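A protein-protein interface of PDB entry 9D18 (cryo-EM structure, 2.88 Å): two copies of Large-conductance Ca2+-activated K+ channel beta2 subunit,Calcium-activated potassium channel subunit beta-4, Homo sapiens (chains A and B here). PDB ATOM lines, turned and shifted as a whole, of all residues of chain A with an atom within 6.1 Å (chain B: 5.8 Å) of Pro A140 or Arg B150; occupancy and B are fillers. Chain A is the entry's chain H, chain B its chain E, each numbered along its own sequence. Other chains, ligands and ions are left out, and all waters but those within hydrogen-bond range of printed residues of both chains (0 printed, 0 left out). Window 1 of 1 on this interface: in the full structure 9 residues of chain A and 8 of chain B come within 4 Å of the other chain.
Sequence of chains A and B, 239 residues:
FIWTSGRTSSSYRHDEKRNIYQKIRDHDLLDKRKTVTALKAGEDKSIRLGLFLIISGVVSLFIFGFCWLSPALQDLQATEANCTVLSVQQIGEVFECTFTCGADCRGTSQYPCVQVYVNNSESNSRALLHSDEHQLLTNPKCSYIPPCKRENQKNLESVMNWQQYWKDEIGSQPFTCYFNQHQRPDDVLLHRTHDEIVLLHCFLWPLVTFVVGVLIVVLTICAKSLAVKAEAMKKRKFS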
ATOM      1  N   GLN A 115     -19.134   8.707 -25.465  1.00  0.00           N
ATOM      2  CA  GLN A 115     -17.705   8.440 -25.417  1.00  0.00           C
ATOM      3  C   GLN A 115     -17.139   8.475 -26.833  1.00  0.00           C
ATOM      4  O   GLN A 115     -17.798   8.082 -27.796  1.00  0.00           O
ATOM      5  CB  GLN A 115     -17.412   7.119 -24.709  1.00  0.00           C
ATOM      6  CG  GLN A 115     -17.689   7.204 -23.200  1.00  0.00           C
ATOM      7  CD  GLN A 115     -17.177   5.979 -22.444  1.00  0.00           C
ATOM      8  OE1 GLN A 115     -16.813   4.962 -23.017  1.00  0.00           O
ATOM      9  NE2 GLN A 115     -17.107   6.022 -21.132  1.00  0.00           N
ATOM     10  N   LEU A 128      -9.351   7.760 -24.645  1.00  0.00           N
ATOM     11  CA  LEU A 128     -10.663   8.418 -24.610  1.00  0.00           C
ATOM     12  C   LEU A 128     -10.494   9.931 -24.750  1.00  0.00           C
ATOM     13  O   LEU A 128      -9.726  10.561 -24.024  1.00  0.00           O
ATOM     14  CB  LEU A 128     -11.361   8.026 -23.298  1.00  0.00           C
ATOM     15  CG  LEU A 128     -12.662   8.776 -22.945  1.00  0.00           C
ATOM     16  CD1 LEU A 128     -13.740   8.710 -24.020  1.00  0.00           C
ATOM     17  CD2 LEU A 128     -13.261   8.152 -21.689  1.00  0.00           C
ATOM     18  N   HIS A 130     -11.511  13.837 -24.385  1.00  0.00           N
ATOM     19  CA  HIS A 130     -12.093  14.737 -23.428  1.00  0.00           C
ATOM     20  C   HIS A 130     -11.880  16.158 -23.922  1.00  0.00           C
ATOM     21  O   HIS A 130     -10.801  16.532 -24.127  1.00  0.00           O
ATOM     22  CB  HIS A 130     -11.428  14.531 -22.097  1.00  0.00           C
ATOM     23  CG  HIS A 130     -11.839  13.317 -21.354  1.00  0.00           C
ATOM     24  ND1 HIS A 130     -13.003  13.164 -20.677  1.00  0.00           N
ATOM     25  CD2 HIS A 130     -11.169  12.146 -21.255  1.00  0.00           C
ATOM     26  CE1 HIS A 130     -13.022  11.952 -20.140  1.00  0.00           C
ATOM     27  NE2 HIS A 130     -11.916  11.288 -20.456  1.00  0.00           N
ATOM     28  N   GLN A 135     -13.403  19.443 -18.527  1.00  0.00           N
ATOM     29  CA  GLN A 135     -14.334  18.373 -18.868  1.00  0.00           C
ATOM     30  C   GLN A 135     -13.837  17.021 -18.340  1.00  0.00           C
ATOM     31  O   GLN A 135     -14.596  16.312 -17.678  1.00  0.00           O
ATOM     32  CB  GLN A 135     -14.610  18.364 -20.378  1.00  0.00           C
ATOM     33  CG  GLN A 135     -15.822  17.496 -20.742  1.00  0.00           C
ATOM     34  CD  GLN A 135     -15.576  15.996 -20.645  1.00  0.00           C
ATOM     35  OE1 GLN A 135     -14.527  15.487 -20.994  1.00  0.00           O
ATOM     36  NE2 GLN A 135     -16.526  15.226 -20.162  1.00  0.00           N
ATOM     37  N   LEU A 136     -12.555  16.698 -18.544  1.00  0.00           N
ATOM     38  CA  LEU A 136     -11.935  15.495 -17.986  1.00  0.00           C
ATOM     39  C   LEU A 136     -12.151  15.414 -16.474  1.00  0.00           C
ATOM     40  O   LEU A 136     -12.511  14.365 -15.966  1.00  0.00           O
ATOM     41  CB  LEU A 136     -10.436  15.472 -18.337  1.00  0.00           C
ATOM     42  CG  LEU A 136      -9.593  14.430 -17.581  1.00  0.00           C
ATOM     43  CD1 LEU A 136     -10.021  12.997 -17.856  1.00  0.00           C
ATOM     44  CD2 LEU A 136      -8.128  14.556 -17.988  1.00  0.00           C
ATOM     45  N   LEU A 137     -11.951  16.506 -15.738  1.00  0.00           N
ATOM     46  CA  LEU A 137     -12.054  16.483 -14.284  1.00  0.00           C
ATOM     47  C   LEU A 137     -13.496  16.592 -13.764  1.00  0.00           C
ATOM     48  O   LEU A 137     -13.797  16.025 -12.717  1.00  0.00           O
ATOM     49  CB  LEU A 137     -11.121  17.561 -13.721  1.00  0.00           C
ATOM     50  CG  LEU A 137      -9.624  17.248 -13.919  1.00  0.00           C
ATOM     51  CD1 LEU A 137      -8.786  18.444 -13.477  1.00  0.00           C
ATOM     52  CD2 LEU A 137      -9.179  16.035 -13.101  1.00  0.00           C
ATOM     53  N   THR A 138     -14.416  17.272 -14.457  1.00  0.00           N
ATOM     54  CA  THR A 138     -15.826  17.355 -14.031  1.00  0.00           C
ATOM     55  C   THR A 138     -16.599  16.056 -14.282  1.00  0.00           C
ATOM     56  O   THR A 138     -17.492  15.718 -13.507  1.00  0.00           O
ATOM     57  CB  THR A 138     -16.543  18.576 -14.638  1.00  0.00           C
ATOM     58  OG1 THR A 138     -17.685  18.885 -13.871  1.00  0.00           O
ATOM     59  CG2 THR A 138     -17.047  18.382 -16.064  1.00  0.00           C
ATOM     60  N   ASN A 139     -16.238  15.283 -15.317  1.00  0.00           N
ATOM     61  CA  ASN A 139     -16.798  13.954 -15.572  1.00  0.00           C
ATOM     62  C   ASN A 139     -15.813  13.057 -16.360  1.00  0.00           C
ATOM     63  O   ASN A 139     -15.966  12.876 -17.568  1.00  0.00           O
ATOM     64  CB  ASN A 139     -18.160  14.093 -16.275  1.00  0.00           C
ATOM     65  CG  ASN A 139     -18.897  12.766 -16.340  1.00  0.00           C
ATOM     66  OD1 ASN A 139     -18.375  11.715 -16.013  1.00  0.00           O
ATOM     67  ND2 ASN A 139     -20.143  12.775 -16.736  1.00  0.00           N
ATOM     68  N   PRO A 140     -14.824  12.432 -15.699  1.00  0.00           N
ATOM     69  CA  PRO A 140     -13.813  11.601 -16.363  1.00  0.00           C
ATOM     70  C   PRO A 140     -14.374  10.324 -16.988  1.00  0.00           C
ATOM     71  O   PRO A 140     -13.746   9.720 -17.854  1.00  0.00           O
ATOM     72  CB  PRO A 140     -12.786  11.265 -15.283  1.00  0.00           C
ATOM     73  CG  PRO A 140     -13.558  11.434 -13.977  1.00  0.00           C
ATOM     74  CD  PRO A 140     -14.553  12.543 -14.278  1.00  0.00           C
ATOM     75  N   LYS A 141     -15.571   9.912 -16.575  1.00  0.00           N
ATOM     76  CA  LYS A 141     -16.341   8.791 -17.124  1.00  0.00           C
ATOM     77  C   LYS A 141     -16.951   9.106 -18.507  1.00  0.00           C
ATOM     78  O   LYS A 141     -17.400   8.183 -19.185  1.00  0.00           O
ATOM     79  CB  LYS A 141     -17.354   8.432 -16.014  1.00  0.00           C
ATOM     80  CG  LYS A 141     -18.612   7.637 -16.344  1.00  0.00           C
ATOM     81  CD  LYS A 141     -18.437   6.127 -16.556  1.00  0.00           C
ATOM     82  CE  LYS A 141     -19.873   5.585 -16.588  1.00  0.00           C
ATOM     83  NZ  LYS A 141     -20.000   4.111 -16.620  1.00  0.00           N
ATOM     84  N   CYS A 142     -16.938  10.363 -18.967  1.00  0.00           N
ATOM     85  CA  CYS A 142     -17.647  10.801 -20.175  1.00  0.00           C
ATOM     86  C   CYS A 142     -16.845  11.783 -21.057  1.00  0.00           C
ATOM     87  O   CYS A 142     -15.971  12.480 -20.558  1.00  0.00           O
ATOM     88  CB  CYS A 142     -18.977  11.409 -19.722  1.00  0.00           C
ATOM     89  SG  CYS A 142     -20.184  11.440 -21.048  1.00  0.00           S
ATOM     90  N   SER A 143     -17.116  11.863 -22.368  1.00  0.00           N
ATOM     91  CA  SER A 143     -16.262  12.591 -23.336  1.00  0.00           C
ATOM     92  C   SER A 143     -16.618  14.066 -23.588  1.00  0.00           C
ATOM     93  O   SER A 143     -15.764  14.863 -23.973  1.00  0.00           O
ATOM     94  CB  SER A 143     -16.293  11.821 -24.654  1.00  0.00           C
ATOM     95  OG  SER A 143     -15.487  12.404 -25.641  1.00  0.00           O
ATOM     96  N   ASP A 186      -4.498   7.264 -20.623  1.00  0.00           N
ATOM     97  CA  ASP A 186      -5.391   6.853 -21.709  1.00  0.00           C
ATOM     98  C   ASP A 186      -6.508   7.891 -21.953  1.00  0.00           C
ATOM     99  O   ASP A 186      -7.608   7.550 -22.388  1.00  0.00           O
ATOM    100  CB  ASP A 186      -5.893   5.409 -21.502  1.00  0.00           C
ATOM    101  CG  ASP A 186      -6.568   5.090 -20.155  1.00  0.00           C
ATOM    102  OD1 ASP A 186      -6.805   5.994 -19.326  1.00  0.00           O
ATOM    103  OD2 ASP A 186      -6.852   3.889 -19.923  1.00  0.00           O
ATOM    104  N   ASP A 187      -6.201   9.174 -21.718  1.00  0.00           N
ATOM    105  CA  ASP A 187      -7.102  10.322 -21.898  1.00  0.00           C
ATOM    106  C   ASP A 187      -6.468  11.393 -22.807  1.00  0.00           C
ATOM    107  O   ASP A 187      -5.280  11.680 -22.694  1.00  0.00           O
ATOM    108  CB  ASP A 187      -7.506  10.943 -20.549  1.00  0.00           C
ATOM    109  CG  ASP A 187      -8.462  10.101 -19.695  1.00  0.00           C
ATOM    110  OD1 ASP A 187      -9.065   9.148 -20.232  1.00  0.00           O
ATOM    111  OD2 ASP A 187      -8.563  10.366 -18.479  1.00  0.00           O
ATOM    112  N   PHE B  99     -12.712   5.525  -9.153  1.00  0.00           N
ATOM    113  CA  PHE B  99     -11.565   5.456 -10.062  1.00  0.00           C
ATOM    114  C   PHE B  99     -10.902   6.826 -10.197  1.00  0.00           C
ATOM    115  O   PHE B  99     -11.561   7.861 -10.121  1.00  0.00           O
ATOM    116  CB  PHE B  99     -11.967   4.882 -11.426  1.00  0.00           C
ATOM    117  CG  PHE B  99     -12.820   5.785 -12.291  1.00  0.00           C
ATOM    118  CD1 PHE B  99     -14.212   5.817 -12.106  1.00  0.00           C
ATOM    119  CD2 PHE B  99     -12.233   6.565 -13.305  1.00  0.00           C
ATOM    120  CE1 PHE B  99     -15.011   6.619 -12.933  1.00  0.00           C
ATOM    121  CE2 PHE B  99     -13.036   7.353 -14.143  1.00  0.00           C
ATOM    122  CZ  PHE B  99     -14.427   7.377 -13.961  1.00  0.00           C
ATOM    123  N   THR B 100      -9.584   6.833 -10.361  1.00  0.00           N
ATOM    124  CA  THR B 100      -8.728   8.013 -10.175  1.00  0.00           C
ATOM    125  C   THR B 100      -7.954   8.362 -11.446  1.00  0.00           C
ATOM    126  O   THR B 100      -7.655   7.503 -12.267  1.00  0.00           O
ATOM    127  CB  THR B 100      -7.781   7.817  -8.987  1.00  0.00           C
ATOM    128  OG1 THR B 100      -6.970   6.690  -9.162  1.00  0.00           O
ATOM    129  CG2 THR B 100      -8.532   7.626  -7.683  1.00  0.00           C
ATOM    130  N   CYS B 101      -7.648   9.662 -11.595  1.00  0.00           N
ATOM    131  CA  CYS B 101      -6.951  10.192 -12.782  1.00  0.00           C
ATOM    132  C   CYS B 101      -6.054  11.452 -12.657  1.00  0.00           C
ATOM    133  O   CYS B 101      -6.213  12.380 -13.451  1.00  0.00           O
ATOM    134  CB  CYS B 101      -7.973  10.466 -13.904  1.00  0.00           C
ATOM    135  SG  CYS B 101      -9.365  11.555 -13.481  1.00  0.00           S
ATOM    136  N   CYS B 105      -9.196  14.193  -9.530  1.00  0.00           N
ATOM    137  CA  CYS B 105      -9.969  13.968 -10.761  1.00  0.00           C
ATOM    138  C   CYS B 105     -11.165  13.003 -10.630  1.00  0.00           C
ATOM    139  O   CYS B 105     -11.937  12.833 -11.569  1.00  0.00           O
ATOM    140  CB  CYS B 105      -8.949  13.532 -11.820  1.00  0.00           C
ATOM    141  SG  CYS B 105      -9.527  13.095 -13.471  1.00  0.00           S
ATOM    142  N   ARG B 106     -11.290  12.305  -9.498  1.00  0.00           N
ATOM    143  CA  ARG B 106     -12.023  11.034  -9.381  1.00  0.00           C
ATOM    144  C   ARG B 106     -13.499  11.040  -9.808  1.00  0.00           C
ATOM    145  O   ARG B 106     -14.205  12.038  -9.649  1.00  0.00           O
ATOM    146  CB  ARG B 106     -11.825  10.453  -7.968  1.00  0.00           C
ATOM    147  CG  ARG B 106     -12.417  11.223  -6.773  1.00  0.00           C
ATOM    148  CD  ARG B 106     -12.104  10.644  -5.389  1.00  0.00           C
ATOM    149  NE  ARG B 106     -12.745  11.410  -4.305  1.00  0.00           N
ATOM    150  CZ  ARG B 106     -12.303  12.512  -3.737  1.00  0.00           C
ATOM    151  NH1 ARG B 106     -12.910  12.995  -2.691  1.00  0.00           N
ATOM    152  NH2 ARG B 106     -11.276  13.164  -4.187  1.00  0.00           N
ATOM    153  N   GLY B 107     -13.976   9.883 -10.255  1.00  0.00           N
ATOM    154  CA  GLY B 107     -15.395   9.561 -10.471  1.00  0.00           C
ATOM    155  C   GLY B 107     -15.736   8.160  -9.956  1.00  0.00           C
ATOM    156  O   GLY B 107     -14.859   7.477  -9.427  1.00  0.00           O
ATOM    157  N   THR B 108     -16.981   7.699 -10.107  1.00  0.00           N
ATOM    158  CA  THR B 108     -17.388   6.359  -9.637  1.00  0.00           C
ATOM    159  C   THR B 108     -17.919   5.451 -10.741  1.00  0.00           C
ATOM    160  O   THR B 108     -18.522   5.889 -11.726  1.00  0.00           O
ATOM    161  CB  THR B 108     -18.360   6.391  -8.447  1.00  0.00           C
ATOM    162  OG1 THR B 108     -19.622   6.890  -8.808  1.00  0.00           O
ATOM    163  CG2 THR B 108     -17.843   7.226  -7.280  1.00  0.00           C
ATOM    164  N   SER B 109     -17.682   4.155 -10.562  1.00  0.00           N
ATOM    165  CA  SER B 109     -18.089   3.077 -11.462  1.00  0.00           C
ATOM    166  C   SER B 109     -18.667   1.924 -10.661  1.00  0.00           C
ATOM    167  O   SER B 109     -18.220   1.649  -9.548  1.00  0.00           O
ATOM    168  CB  SER B 109     -16.903   2.589 -12.288  1.00  0.00           C
ATOM    169  OG  SER B 109     -16.433   3.617 -13.127  1.00  0.00           O
ATOM    170  N   CYS B 148     -10.723  -0.385  -9.152  1.00  0.00           N
ATOM    171  CA  CYS B 148     -11.484   0.381 -10.121  1.00  0.00           C
ATOM    172  C   CYS B 148     -10.646   0.827 -11.311  1.00  0.00           C
ATOM    173  O   CYS B 148      -9.760   1.672 -11.181  1.00  0.00           O
ATOM    174  CB  CYS B 148     -12.112   1.587  -9.422  1.00  0.00           C
ATOM    175  SG  CYS B 148     -13.348   1.197  -8.163  1.00  0.00           S
ATOM    176  N   LYS B 149     -10.981   0.250 -12.464  1.00  0.00           N
ATOM    177  CA  LYS B 149     -10.308   0.523 -13.723  1.00  0.00           C
ATOM    178  C   LYS B 149     -11.251   1.093 -14.784  1.00  0.00           C
ATOM    179  O   LYS B 149     -11.624   0.402 -15.734  1.00  0.00           O
ATOM    180  CB  LYS B 149      -9.639  -0.747 -14.252  1.00  0.00           C
ATOM    181  CG  LYS B 149      -8.512  -1.264 -13.375  1.00  0.00           C
ATOM    182  CD  LYS B 149      -7.895  -2.523 -13.961  1.00  0.00           C
ATOM    183  CE  LYS B 149      -6.800  -3.071 -13.060  1.00  0.00           C
ATOM    184  NZ  LYS B 149      -5.665  -2.115 -12.925  1.00  0.00           N
ATOM    185  N   ARG B 150     -11.637   2.350 -14.570  1.00  0.00           N
ATOM    186  CA  ARG B 150     -12.526   3.127 -15.444  1.00  0.00           C
ATOM    187  C   ARG B 150     -13.964   2.619 -15.624  1.00  0.00           C
ATOM    188  O   ARG B 150     -14.824   2.867 -14.780  1.00  0.00           O
ATOM    189  CB  ARG B 150     -11.873   3.418 -16.805  1.00  0.00           C
ATOM    190  CG  ARG B 150     -10.605   4.253 -16.719  1.00  0.00           C
ATOM    191  CD  ARG B 150     -10.891   5.644 -16.177  1.00  0.00           C
ATOM    192  NE  ARG B 150     -11.815   6.381 -17.033  1.00  0.00           N
ATOM    193  CZ  ARG B 150     -11.453   7.032 -18.134  1.00  0.00           C
ATOM    194  NH1 ARG B 150     -12.362   7.674 -18.854  1.00  0.00           N
ATOM    195  NH2 ARG B 150     -10.183   7.042 -18.515  1.00  0.00           N
ATOM    196  N   GLU B 151     -14.215   1.916 -16.722  1.00  0.00           N
ATOM    197  CA  GLU B 151     -15.563   1.442 -17.051  1.00  0.00           C
ATOM    198  C   GLU B 151     -16.084   0.175 -16.363  1.00  0.00           C
ATOM    199  O   GLU B 151     -15.342  -0.763 -16.080  1.00  0.00           O
ATOM    200  CB  GLU B 151     -15.707   1.292 -18.569  1.00  0.00           C
ATOM    201  CG  GLU B 151     -14.714   0.328 -19.195  1.00  0.00           C
ATOM    202  CD  GLU B 151     -13.487   1.031 -19.742  1.00  0.00           C
ATOM    203  OE1 GLU B 151     -13.591   2.226 -20.092  1.00  0.00           O
ATOM    204  OE2 GLU B 151     -12.420   0.389 -19.823  1.00  0.00           O
ATOM    205  N   ASN B 152     -17.393   0.186 -16.122  1.00  0.00           N
ATOM    206  CA  ASN B 152     -18.145  -0.916 -15.512  1.00  0.00           C
ATOM    207  C   ASN B 152     -17.830  -2.294 -16.109  1.00  0.00           C
ATOM    208  O   ASN B 152     -17.747  -3.281 -15.380  1.00  0.00           O
ATOM    209  CB  ASN B 152     -19.646  -0.633 -15.658  1.00  0.00           C
ATOM    210  CG  ASN B 152     -20.165   0.521 -14.825  1.00  0.00           C
ATOM    211  OD1 ASN B 152     -19.439   1.230 -14.145  1.00  0.00           O
ATOM    212  ND2 ASN B 152     -21.455   0.736 -14.840  1.00  0.00           N
ATOM    213  N   ASN B 155     -14.664  -3.769 -14.514  1.00  0.00           N
ATOM    214  CA  ASN B 155     -14.970  -4.198 -13.148  1.00  0.00           C
ATOM    215  C   ASN B 155     -15.719  -5.537 -13.145  1.00  0.00           C
ATOM    216  O   ASN B 155     -15.318  -6.459 -12.441  1.00  0.00           O
ATOM    217  CB  ASN B 155     -15.788  -3.124 -12.424  1.00  0.00           C
ATOM    218  CG  ASN B 155     -15.040  -1.847 -12.129  1.00  0.00           C
ATOM    219  OD1 ASN B 155     -13.828  -1.762 -12.207  1.00  0.00           O
ATOM    220  ND2 ASN B 155     -15.754  -0.820 -11.753  1.00  0.00           N
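Among the printed residues, merely in contact across the chains: Leu A137 with Cys B105, Leu A128 with Arg B150, Pro A140 with Cys B105, Lys A141 with Phe B99, Lys A141 with Asn B152, Pro A140 with Cys B101 and His A130 with Arg B150.
No position is printed for both chains.
Of the 10 pairs that touch across the chains among the printed residues, none has its exchanged pair printed and touching as well.
The guanidinium group (NH1) of Arg B150 is in hydrogen-bond range of the backbone carbonyl oxygen (O) of Pro A140, 2.7 Å away.
The side-chain carboxylate of Asp A186 lies within salt-bridge range of the guanidinium group of Arg B150 (3.6 Å).
NH2 of Arg B150 is in salt-bridge range of OD1 of Asp A187, at 2.9 Å.
Of the 14 printed residues of chain B, 5 touch a printed residue of chain A.
Printed residues of chain B that touch a printed residue of chain A: Phe B99, Cys B101, Cys B105, Arg B150 and Asn B152.
Of the 14 printed residues of chain A, 7 touch a printed residue of chain B.
Printed residues of chain A that touch a printed residue of chain B: Leu A128, His A130, Leu A137, Pro A140, Lys A141, Asp A186 and Asp A187.
Among the printed residues, Asp or Glu carboxylates within 4 Å of a Lys or Arg side-chain nitrogen of the other chain: Asp A186 with Arg B150 and Asp A187 with Arg B150.
OG of Ser B109 lies within hydrogen-bond range of O of Arg B150 (2.4 Å).
The backbone carbonyl oxygen (O) of Lys A141 is in hydrogen-bond range of the side-chain amide nitrogen (NE2) of Gln A115, at 2.9 Å.
The backbone NH (N) of Leu A128 is in hydrogen-bond range of the backbone carbonyl oxygen (O) of Asp A186, at 2.9 Å.
The side-chain amide oxygen of Gln A135 lies within hydrogen-bond range of a ring nitrogen (ND1) of His A130, 2.8 Å away.
A ring nitrogen (ND1) of His A130 lies close to the backbone carbonyl oxygen (O) of Cys A142 (3.0 Å).
OD1 of Asn A139 sits close to N of Lys A141 (3.4 Å).
Of the printed residues of chain B, His A130 touches Arg B150 (3.98 Å).
Printed residues of chain B within 4 Å of Leu A137: Cys B105 (2.8 Å).
Of chain B, only Cys B101, Cys B105 and Arg B150 come within 4 Å of Pro A140.
Printed residues of chain A within 4 Å of Cys B101: Pro A140 (3.9 Å).
Arg B150 touches just these residues of chain A: Leu A128, His A130, Pro A140, Asp A186 and Asp A187.
The nearest residue of chain A that does not touch Arg B150 is Lys A141 (4.5 Å).
The nearest printed residue of chain B that does not touch Leu A128 is Glu B151 (6.1 Å).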
